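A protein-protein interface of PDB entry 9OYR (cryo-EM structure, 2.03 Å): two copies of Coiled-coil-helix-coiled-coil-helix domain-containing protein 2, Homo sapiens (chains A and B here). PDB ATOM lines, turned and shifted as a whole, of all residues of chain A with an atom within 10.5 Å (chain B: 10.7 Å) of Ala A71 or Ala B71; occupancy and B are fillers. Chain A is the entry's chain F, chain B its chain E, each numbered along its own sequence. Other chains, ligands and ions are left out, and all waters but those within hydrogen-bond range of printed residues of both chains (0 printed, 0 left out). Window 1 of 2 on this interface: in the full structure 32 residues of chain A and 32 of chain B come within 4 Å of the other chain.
The backbone NH of Leu B55 sits at hydrogen-bond distance from the backbone carbonyl oxygen of Gly A54 (2.8 Å).
N of Met A56 is in hydrogen-bond range of O of Leu B55, at 2.8 Å.
N of Ala B57 is in hydrogen-bond range of O of Met A56, at 3.1 Å.
The backbone NH (N) of Ala B67 lies within hydrogen-bond range of the backbone carbonyl oxygen (O) of Val A66 (2.8 Å).
The backbone carbonyl oxygen (O) of Ala B67 lies within hydrogen-bond range of the backbone NH (N) of Val A68 (2.9 Å).
The backbone NH of Gly B69 lies within hydrogen-bond range of the side-chain sulfur of Met A59, at 3.3 Å.
N of Gly B69 lies within hydrogen-bond range of O of Val A68 (2.9 Å).
N of Gly B69 lies close to O of Gly A69, at 3.4 Å.
O of Met A56 sits at hydrogen-bond distance from OG of Ser B70 (3.0 Å).
The backbone carbonyl oxygen (O) of Gly A69 is in hydrogen-bond range of the backbone NH (N) of Ser B70, at 2.8 Å.
N of Ala A71 is in hydrogen-bond range of O of Ser B70 (3.1 Å).
The backbone carbonyl oxygen (O) of Ala A71 is in hydrogen-bond range of the backbone NH (N) of Val B72.
The backbone NH of Gly A73 is in hydrogen-bond range of the backbone carbonyl oxygen of Val B72, 2.9 Å away.
The backbone carbonyl oxygen (O) of Gly A73 lies within hydrogen-bond range of the backbone NH (N) of His B74.
Among the printed residues, pairs that only touch across the chains: His A74 with His B74 (3.0 Å), Gly A73 with Gly B73 (3.1 Å), Ala A71 with Ala B71 (3.1 Å), Ser A70 with Ser B70 (3.2 Å), Val A72 with Val B72 (3.2 Å), Val A68 with Val B68 (3.2 Å), Met A59 with Met B59 (3.3 Å), Ala A67 with Ala B67 (3.3 Å), Ala A57 with Ala B57 (3.3 Å), Met A56 with Met B56 (3.3 Å), Gly A54 with Gly B54 (3.4 Å), Val A66 with Val B66 (3.4 Å), Leu A55 with Ser B70 (3.4 Å), Leu A55 with Leu B55 (3.4 Å), Met A59 with Ala B67 (3.7 Å), Leu A55 with Ala B71 (3.7 Å) and Ala A57 with Gly B69 (3.9 Å).
Gly A69 touches two residues of chain B.
Of chain B, only Ser B70 (3.2 Å) comes within 4 Å of Ser A70.
Of chain B, only Ser B70, Ala B71 and Val B72 come within 4 Å of Ala A71.
Of the printed residues of chain B, Val A72 touches Val B72 (3.2 Å).
Printed residues of chain B within 4 Å of His A74: His B74 (3.0 Å).
Of the printed residues of chain A, Ala B57 touches Met A56 (3.1 Å) and Ala A57 (3.3 Å).
Of chain A, only Ala A57, Met A59, Val A68 and Gly A69 come within 4 Å of Gly B69.
Ser B70 touches five residues of chain A.
Ala B71 touches just these residues of chain A: Leu A55 and Ala A71.
Val B72 touches three residues of chain A.
The nearest residue of chain B that does not touch Ala A71 is Gly B73 (5.6 Å).
Hydrophobic or aromatic side chains of chain A that line the printed part of chain B: Leu A55, Ala A57, Met A59, Val A72 and His A74.
Of the 14 printed residues of chain B, 14 touch a printed residue of chain A.
Hydrophobic or aromatic side chains of chain B within 4 Å of the printed part of chain A: Val B68, Ala B71 and His B74.
Among the printed residues, 31 pairs touch across the chains.
Among the printed residues, no Asp or Glu carboxylate lies within 4 Å of a Lys or Arg side-chain nitrogen of the other chain.
Gly A54 touches its own counterpart, Gly B54.
Leu A55 touches Ser B70, but with the chains exchanged Ser A70 does not touch Leu B55 (6.2 Å).
Met A56 touches Leu B55, but with the chains exchanged Leu A55 does not touch Met B56 (5.6 Å).
Ala B57 touches its own counterpart, Ala A57.
Positions printed for both chains: 54, 55, 56, 57, 59, 66, 67, 68, 69, 70, 71, 72, 73 and 74.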
ATOM      1  N   GLY A  54      -3.646 -22.659  -4.486  1.00  0.00           N
ATOM      2  CA  GLY A  54      -4.814 -23.311  -5.042  1.00  0.00           C
ATOM      3  C   GLY A  54      -5.929 -23.458  -4.030  1.00  0.00           C
ATOM      4  O   GLY A  54      -6.775 -22.583  -3.910  1.00  0.00           O
ATOM      5  N   LEU A  55      -5.931 -24.572  -3.306  1.00  0.00           N
ATOM      6  CA  LEU A  55      -6.898 -24.836  -2.253  1.00  0.00           C
ATOM      7  C   LEU A  55      -6.152 -24.970  -0.936  1.00  0.00           C
ATOM      8  O   LEU A  55      -5.213 -25.762  -0.831  1.00  0.00           O
ATOM      9  CB  LEU A  55      -7.690 -26.111  -2.532  1.00  0.00           C
ATOM     10  CG  LEU A  55      -8.863 -26.068  -3.510  1.00  0.00           C
ATOM     11  CD1 LEU A  55      -8.367 -26.089  -4.930  1.00  0.00           C
ATOM     12  CD2 LEU A  55      -9.809 -27.224  -3.260  1.00  0.00           C
ATOM     13  N   MET A  56      -6.564 -24.204   0.063  1.00  0.00           N
ATOM     14  CA  MET A  56      -5.994 -24.297   1.397  1.00  0.00           C
ATOM     15  C   MET A  56      -7.122 -24.388   2.410  1.00  0.00           C
ATOM     16  O   MET A  56      -8.136 -23.702   2.279  1.00  0.00           O
ATOM     17  CB  MET A  56      -5.091 -23.102   1.695  1.00  0.00           C
ATOM     18  CG  MET A  56      -4.257 -23.265   2.945  1.00  0.00           C
ATOM     19  SD  MET A  56      -3.451 -21.737   3.450  1.00  0.00           S
ATOM     20  CE  MET A  56      -3.380 -20.857   1.892  1.00  0.00           C
ATOM     21  N   ALA A  57      -6.952 -25.243   3.410  1.00  0.00           N
ATOM     22  CA  ALA A  57      -7.951 -25.395   4.456  1.00  0.00           C
ATOM     23  C   ALA A  57      -7.262 -25.637   5.789  1.00  0.00           C
ATOM     24  O   ALA A  57      -6.362 -26.470   5.879  1.00  0.00           O
ATOM     25  CB  ALA A  57      -8.908 -26.538   4.139  1.00  0.00           C
ATOM     26  N   MET A  59      -8.832 -26.706   9.318  1.00  0.00           N
ATOM     27  CA  MET A  59     -10.101 -27.108   9.902  1.00  0.00           C
ATOM     28  C   MET A  59      -9.872 -27.759  11.250  1.00  0.00           C
ATOM     29  O   MET A  59      -9.028 -28.648  11.382  1.00  0.00           O
ATOM     30  CB  MET A  59     -10.860 -28.077   9.000  1.00  0.00           C
ATOM     31  CG  MET A  59     -11.159 -27.540   7.624  1.00  0.00           C
ATOM     32  SD  MET A  59     -11.712 -28.811   6.488  1.00  0.00           S
ATOM     33  CE  MET A  59     -12.918 -29.669   7.500  1.00  0.00           C
ATOM     34  N   VAL A  66     -18.268 -36.827   7.624  1.00  0.00           N
ATOM     35  CA  VAL A  66     -17.219 -36.728   6.622  1.00  0.00           C
ATOM     36  C   VAL A  66     -16.520 -35.395   6.821  1.00  0.00           C
ATOM     37  O   VAL A  66     -17.177 -34.353   6.880  1.00  0.00           O
ATOM     38  CB  VAL A  66     -17.770 -36.837   5.187  1.00  0.00           C
ATOM     39  CG1 VAL A  66     -16.692 -36.507   4.180  1.00  0.00           C
ATOM     40  CG2 VAL A  66     -18.335 -38.216   4.936  1.00  0.00           C
ATOM     41  N   ALA A  67     -15.198 -35.423   6.927  1.00  0.00           N
ATOM     42  CA  ALA A  67     -14.395 -34.216   7.054  1.00  0.00           C
ATOM     43  C   ALA A  67     -13.349 -34.220   5.954  1.00  0.00           C
ATOM     44  O   ALA A  67     -12.564 -35.165   5.846  1.00  0.00           O
ATOM     45  CB  ALA A  67     -13.735 -34.127   8.432  1.00  0.00           C
ATOM     46  N   VAL A  68     -13.344 -33.178   5.135  1.00  0.00           N
ATOM     47  CA  VAL A  68     -12.427 -33.074   4.013  1.00  0.00           C
ATOM     48  C   VAL A  68     -11.788 -31.699   4.033  1.00  0.00           C
ATOM     49  O   VAL A  68     -12.488 -30.688   4.125  1.00  0.00           O
ATOM     50  CB  VAL A  68     -13.135 -33.318   2.667  1.00  0.00           C
ATOM     51  CG1 VAL A  68     -12.156 -33.167   1.528  1.00  0.00           C
ATOM     52  CG2 VAL A  68     -13.787 -34.686   2.645  1.00  0.00           C
ATOM     53  N   GLY A  69     -10.465 -31.658   3.930  1.00  0.00           N
ATOM     54  CA  GLY A  69      -9.772 -30.393   3.843  1.00  0.00           C
ATOM     55  C   GLY A  69      -9.897 -29.739   2.485  1.00  0.00           C
ATOM     56  O   GLY A  69     -10.582 -28.728   2.339  1.00  0.00           O
ATOM     57  N   SER A  70      -9.260 -30.322   1.479  1.00  0.00           N
ATOM     58  CA  SER A  70      -9.252 -29.778   0.131  1.00  0.00           C
ATOM     59  C   SER A  70      -9.502 -30.916  -0.841  1.00  0.00           C
ATOM     60  O   SER A  70      -8.926 -31.994  -0.689  1.00  0.00           O
ATOM     61  CB  SER A  70      -7.920 -29.090  -0.185  1.00  0.00           C
ATOM     62  OG  SER A  70      -7.681 -28.003   0.682  1.00  0.00           O
ATOM     63  N   ALA A  71     -10.355 -30.686  -1.832  1.00  0.00           N
ATOM     64  CA  ALA A  71     -10.725 -31.763  -2.735  1.00  0.00           C
ATOM     65  C   ALA A  71     -11.142 -31.199  -4.079  1.00  0.00           C
ATOM     66  O   ALA A  71     -11.803 -30.165  -4.148  1.00  0.00           O
ATOM     67  CB  ALA A  71     -11.856 -32.611  -2.150  1.00  0.00           C
ATOM     68  N   VAL A  72     -10.759 -31.895  -5.141  1.00  0.00           N
ATOM     69  CA  VAL A  72     -11.074 -31.499  -6.504  1.00  0.00           C
ATOM     70  C   VAL A  72     -11.570 -32.722  -7.252  1.00  0.00           C
ATOM     71  O   VAL A  72     -10.949 -33.786  -7.189  1.00  0.00           O
ATOM     72  CB  VAL A  72      -9.856 -30.892  -7.226  1.00  0.00           C
ATOM     73  CG1 VAL A  72     -10.185 -30.620  -8.676  1.00  0.00           C
ATOM     74  CG2 VAL A  72      -9.395 -29.634  -6.535  1.00  0.00           C
ATOM     75  N   GLY A  73     -12.678 -32.573  -7.958  1.00  0.00           N
ATOM     76  CA  GLY A  73     -13.132 -33.609  -8.858  1.00  0.00           C
ATOM     77  C   GLY A  73     -13.490 -33.010 -10.191  1.00  0.00           C
ATOM     78  O   GLY A  73     -14.289 -32.076 -10.241  1.00  0.00           O
ATOM     79  N   HIS A  74     -12.901 -33.488 -11.278  1.00  0.00           N
ATOM     80  CA  HIS A  74     -13.238 -32.912 -12.566  1.00  0.00           C
ATOM     81  C   HIS A  74     -13.183 -33.954 -13.667  1.00  0.00           C
ATOM     82  O   HIS A  74     -12.455 -34.939 -13.576  1.00  0.00           O
ATOM     83  CB  HIS A  74     -12.331 -31.723 -12.923  1.00  0.00           C
ATOM     84  CG  HIS A  74     -10.871 -32.008 -12.836  1.00  0.00           C
ATOM     85  ND1 HIS A  74     -10.260 -32.378 -11.659  1.00  0.00           N
ATOM     86  CD2 HIS A  74      -9.902 -32.013 -13.781  1.00  0.00           C
ATOM     87  CE1 HIS A  74      -8.975 -32.583 -11.880  1.00  0.00           C
ATOM     88  NE2 HIS A  74      -8.731 -32.370 -13.160  1.00  0.00           N
ATOM     89  N   GLY B  54      -6.541 -18.868  -4.330  1.00  0.00           N
ATOM     90  CA  GLY B  54      -7.699 -19.512  -4.912  1.00  0.00           C
ATOM     91  C   GLY B  54      -8.829 -19.674  -3.921  1.00  0.00           C
ATOM     92  O   GLY B  54      -9.679 -18.801  -3.803  1.00  0.00           O
ATOM     93  N   LEU B  55      -8.842 -20.798  -3.212  1.00  0.00           N
ATOM     94  CA  LEU B  55      -9.827 -21.077  -2.178  1.00  0.00           C
ATOM     95  C   LEU B  55      -9.101 -21.226  -0.851  1.00  0.00           C
ATOM     96  O   LEU B  55      -8.164 -22.021  -0.743  1.00  0.00           O
ATOM     97  CB  LEU B  55     -10.612 -22.348  -2.488  1.00  0.00           C
ATOM     98  CG  LEU B  55     -11.770 -22.293  -3.483  1.00  0.00           C
ATOM     99  CD1 LEU B  55     -11.251 -22.295  -4.896  1.00  0.00           C
ATOM    100  CD2 LEU B  55     -12.718 -23.453  -3.263  1.00  0.00           C
ATOM    101  N   MET B  56      -9.531 -20.475   0.150  1.00  0.00           N
ATOM    102  CA  MET B  56      -8.981 -20.586   1.492  1.00  0.00           C
ATOM    103  C   MET B  56     -10.124 -20.692   2.486  1.00  0.00           C
ATOM    104  O   MET B  56     -11.137 -20.004   2.348  1.00  0.00           O
ATOM    105  CB  MET B  56      -8.084 -19.396   1.821  1.00  0.00           C
ATOM    106  CG  MET B  56      -7.270 -19.574   3.082  1.00  0.00           C
ATOM    107  SD  MET B  56      -6.473 -18.052   3.620  1.00  0.00           S
ATOM    108  CE  MET B  56      -6.378 -17.151   2.074  1.00  0.00           C
ATOM    109  N   ALA B  57      -9.969 -21.560   3.478  1.00  0.00           N
ATOM    110  CA  ALA B  57     -10.984 -21.725   4.505  1.00  0.00           C
ATOM    111  C   ALA B  57     -10.318 -21.985   5.845  1.00  0.00           C
ATOM    112  O   ALA B  57      -9.417 -22.819   5.939  1.00  0.00           O
ATOM    113  CB  ALA B  57     -11.937 -22.866   4.158  1.00  0.00           C
ATOM    114  N   MET B  59     -11.942 -23.104   9.334  1.00  0.00           N
ATOM    115  CA  MET B  59     -13.220 -23.514   9.893  1.00  0.00           C
ATOM    116  C   MET B  59     -13.011 -24.183  11.236  1.00  0.00           C
ATOM    117  O   MET B  59     -12.168 -25.073  11.369  1.00  0.00           O
ATOM    118  CB  MET B  59     -13.963 -24.471   8.966  1.00  0.00           C
ATOM    119  CG  MET B  59     -14.241 -23.917   7.592  1.00  0.00           C
ATOM    120  SD  MET B  59     -14.775 -25.172   6.431  1.00  0.00           S
ATOM    121  CE  MET B  59     -15.995 -26.045   7.411  1.00  0.00           C
ATOM    122  N   VAL B  66     -21.339 -33.208   7.355  1.00  0.00           N
ATOM    123  CA  VAL B  66     -20.274 -33.095   6.372  1.00  0.00           C
ATOM    124  C   VAL B  66     -19.580 -31.764   6.599  1.00  0.00           C
ATOM    125  O   VAL B  66     -20.239 -30.723   6.661  1.00  0.00           O
ATOM    126  CB  VAL B  66     -20.803 -33.185   4.926  1.00  0.00           C
ATOM    127  CG1 VAL B  66     -19.710 -32.840   3.940  1.00  0.00           C
ATOM    128  CG2 VAL B  66     -21.364 -34.561   4.647  1.00  0.00           C
ATOM    129  N   ALA B  67     -18.260 -31.793   6.726  1.00  0.00           N
ATOM    130  CA  ALA B  67     -17.461 -30.587   6.880  1.00  0.00           C
ATOM    131  C   ALA B  67     -16.397 -30.575   5.798  1.00  0.00           C
ATOM    132  O   ALA B  67     -15.610 -31.518   5.690  1.00  0.00           O
ATOM    133  CB  ALA B  67     -16.822 -30.515   8.271  1.00  0.00           C
ATOM    134  N   VAL B  68     -16.381 -29.523   4.993  1.00  0.00           N
ATOM    135  CA  VAL B  68     -15.446 -29.403   3.888  1.00  0.00           C
ATOM    136  C   VAL B  68     -14.808 -28.026   3.937  1.00  0.00           C
ATOM    137  O   VAL B  68     -15.512 -27.018   4.031  1.00  0.00           O
ATOM    138  CB  VAL B  68     -16.133 -29.629   2.527  1.00  0.00           C
ATOM    139  CG1 VAL B  68     -15.137 -29.461   1.406  1.00  0.00           C
ATOM    140  CG2 VAL B  68     -16.783 -30.997   2.478  1.00  0.00           C
ATOM    141  N   GLY B  69     -13.484 -27.984   3.855  1.00  0.00           N
ATOM    142  CA  GLY B  69     -12.791 -26.718   3.795  1.00  0.00           C
ATOM    143  C   GLY B  69     -12.895 -26.045   2.445  1.00  0.00           C
ATOM    144  O   GLY B  69     -13.578 -25.033   2.302  1.00  0.00           O
ATOM    145  N   SER B  70     -12.242 -26.614   1.441  1.00  0.00           N
ATOM    146  CA  SER B  70     -12.212 -26.052   0.102  1.00  0.00           C
ATOM    147  C   SER B  70     -12.447 -27.177  -0.890  1.00  0.00           C
ATOM    148  O   SER B  70     -11.871 -28.257  -0.744  1.00  0.00           O
ATOM    149  CB  SER B  70     -10.876 -25.359  -0.185  1.00  0.00           C
ATOM    150  OG  SER B  70     -10.653 -24.283   0.702  1.00  0.00           O
ATOM    151  N   ALA B  71     -13.283 -26.935  -1.891  1.00  0.00           N
ATOM    152  CA  ALA B  71     -13.638 -28.000  -2.814  1.00  0.00           C
ATOM    153  C   ALA B  71     -14.034 -27.418  -4.157  1.00  0.00           C
ATOM    154  O   ALA B  71     -14.694 -26.383  -4.223  1.00  0.00           O
ATOM    155  CB  ALA B  71     -14.778 -28.856  -2.259  1.00  0.00           C
ATOM    156  N   VAL B  72     -13.634 -28.099  -5.222  1.00  0.00           N
ATOM    157  CA  VAL B  72     -13.928 -27.685  -6.584  1.00  0.00           C
ATOM    158  C   VAL B  72     -14.410 -28.899  -7.356  1.00  0.00           C
ATOM    159  O   VAL B  72     -13.789 -29.962  -7.298  1.00  0.00           O
ATOM    160  CB  VAL B  72     -12.698 -27.067  -7.279  1.00  0.00           C
ATOM    161  CG1 VAL B  72     -13.005 -26.776  -8.730  1.00  0.00           C
ATOM    162  CG2 VAL B  72     -12.249 -25.818  -6.564  1.00  0.00           C
ATOM    163  N   GLY B  73     -15.507 -28.741  -8.079  1.00  0.00           N
ATOM    164  CA  GLY B  73     -15.945 -29.765  -8.998  1.00  0.00           C
ATOM    165  C   GLY B  73     -16.283 -29.148 -10.330  1.00  0.00           C
ATOM    166  O   GLY B  73     -17.081 -28.214 -10.380  1.00  0.00           O
ATOM    167  N   HIS B  74     -15.677 -29.611 -11.413  1.00  0.00           N
ATOM    168  CA  HIS B  74     -15.994 -29.017 -12.699  1.00  0.00           C
ATOM    169  C   HIS B  74     -15.920 -30.044 -13.813  1.00  0.00           C
ATOM    170  O   HIS B  74     -15.193 -31.030 -13.723  1.00  0.00           O
ATOM    171  CB  HIS B  74     -15.083 -27.823 -13.024  1.00  0.00           C
ATOM    172  CG  HIS B  74     -13.624 -28.109 -12.919  1.00  0.00           C
ATOM    173  ND1 HIS B  74     -13.031 -28.494 -11.738  1.00  0.00           N
ATOM    174  CD2 HIS B  74     -12.640 -28.099 -13.849  1.00  0.00           C
ATOM    175  CE1 HIS B  74     -11.742 -28.695 -11.940  1.00  0.00           C
ATOM    176  NE2 HIS B  74     -11.478 -28.464 -13.213  1.00  0.00           N
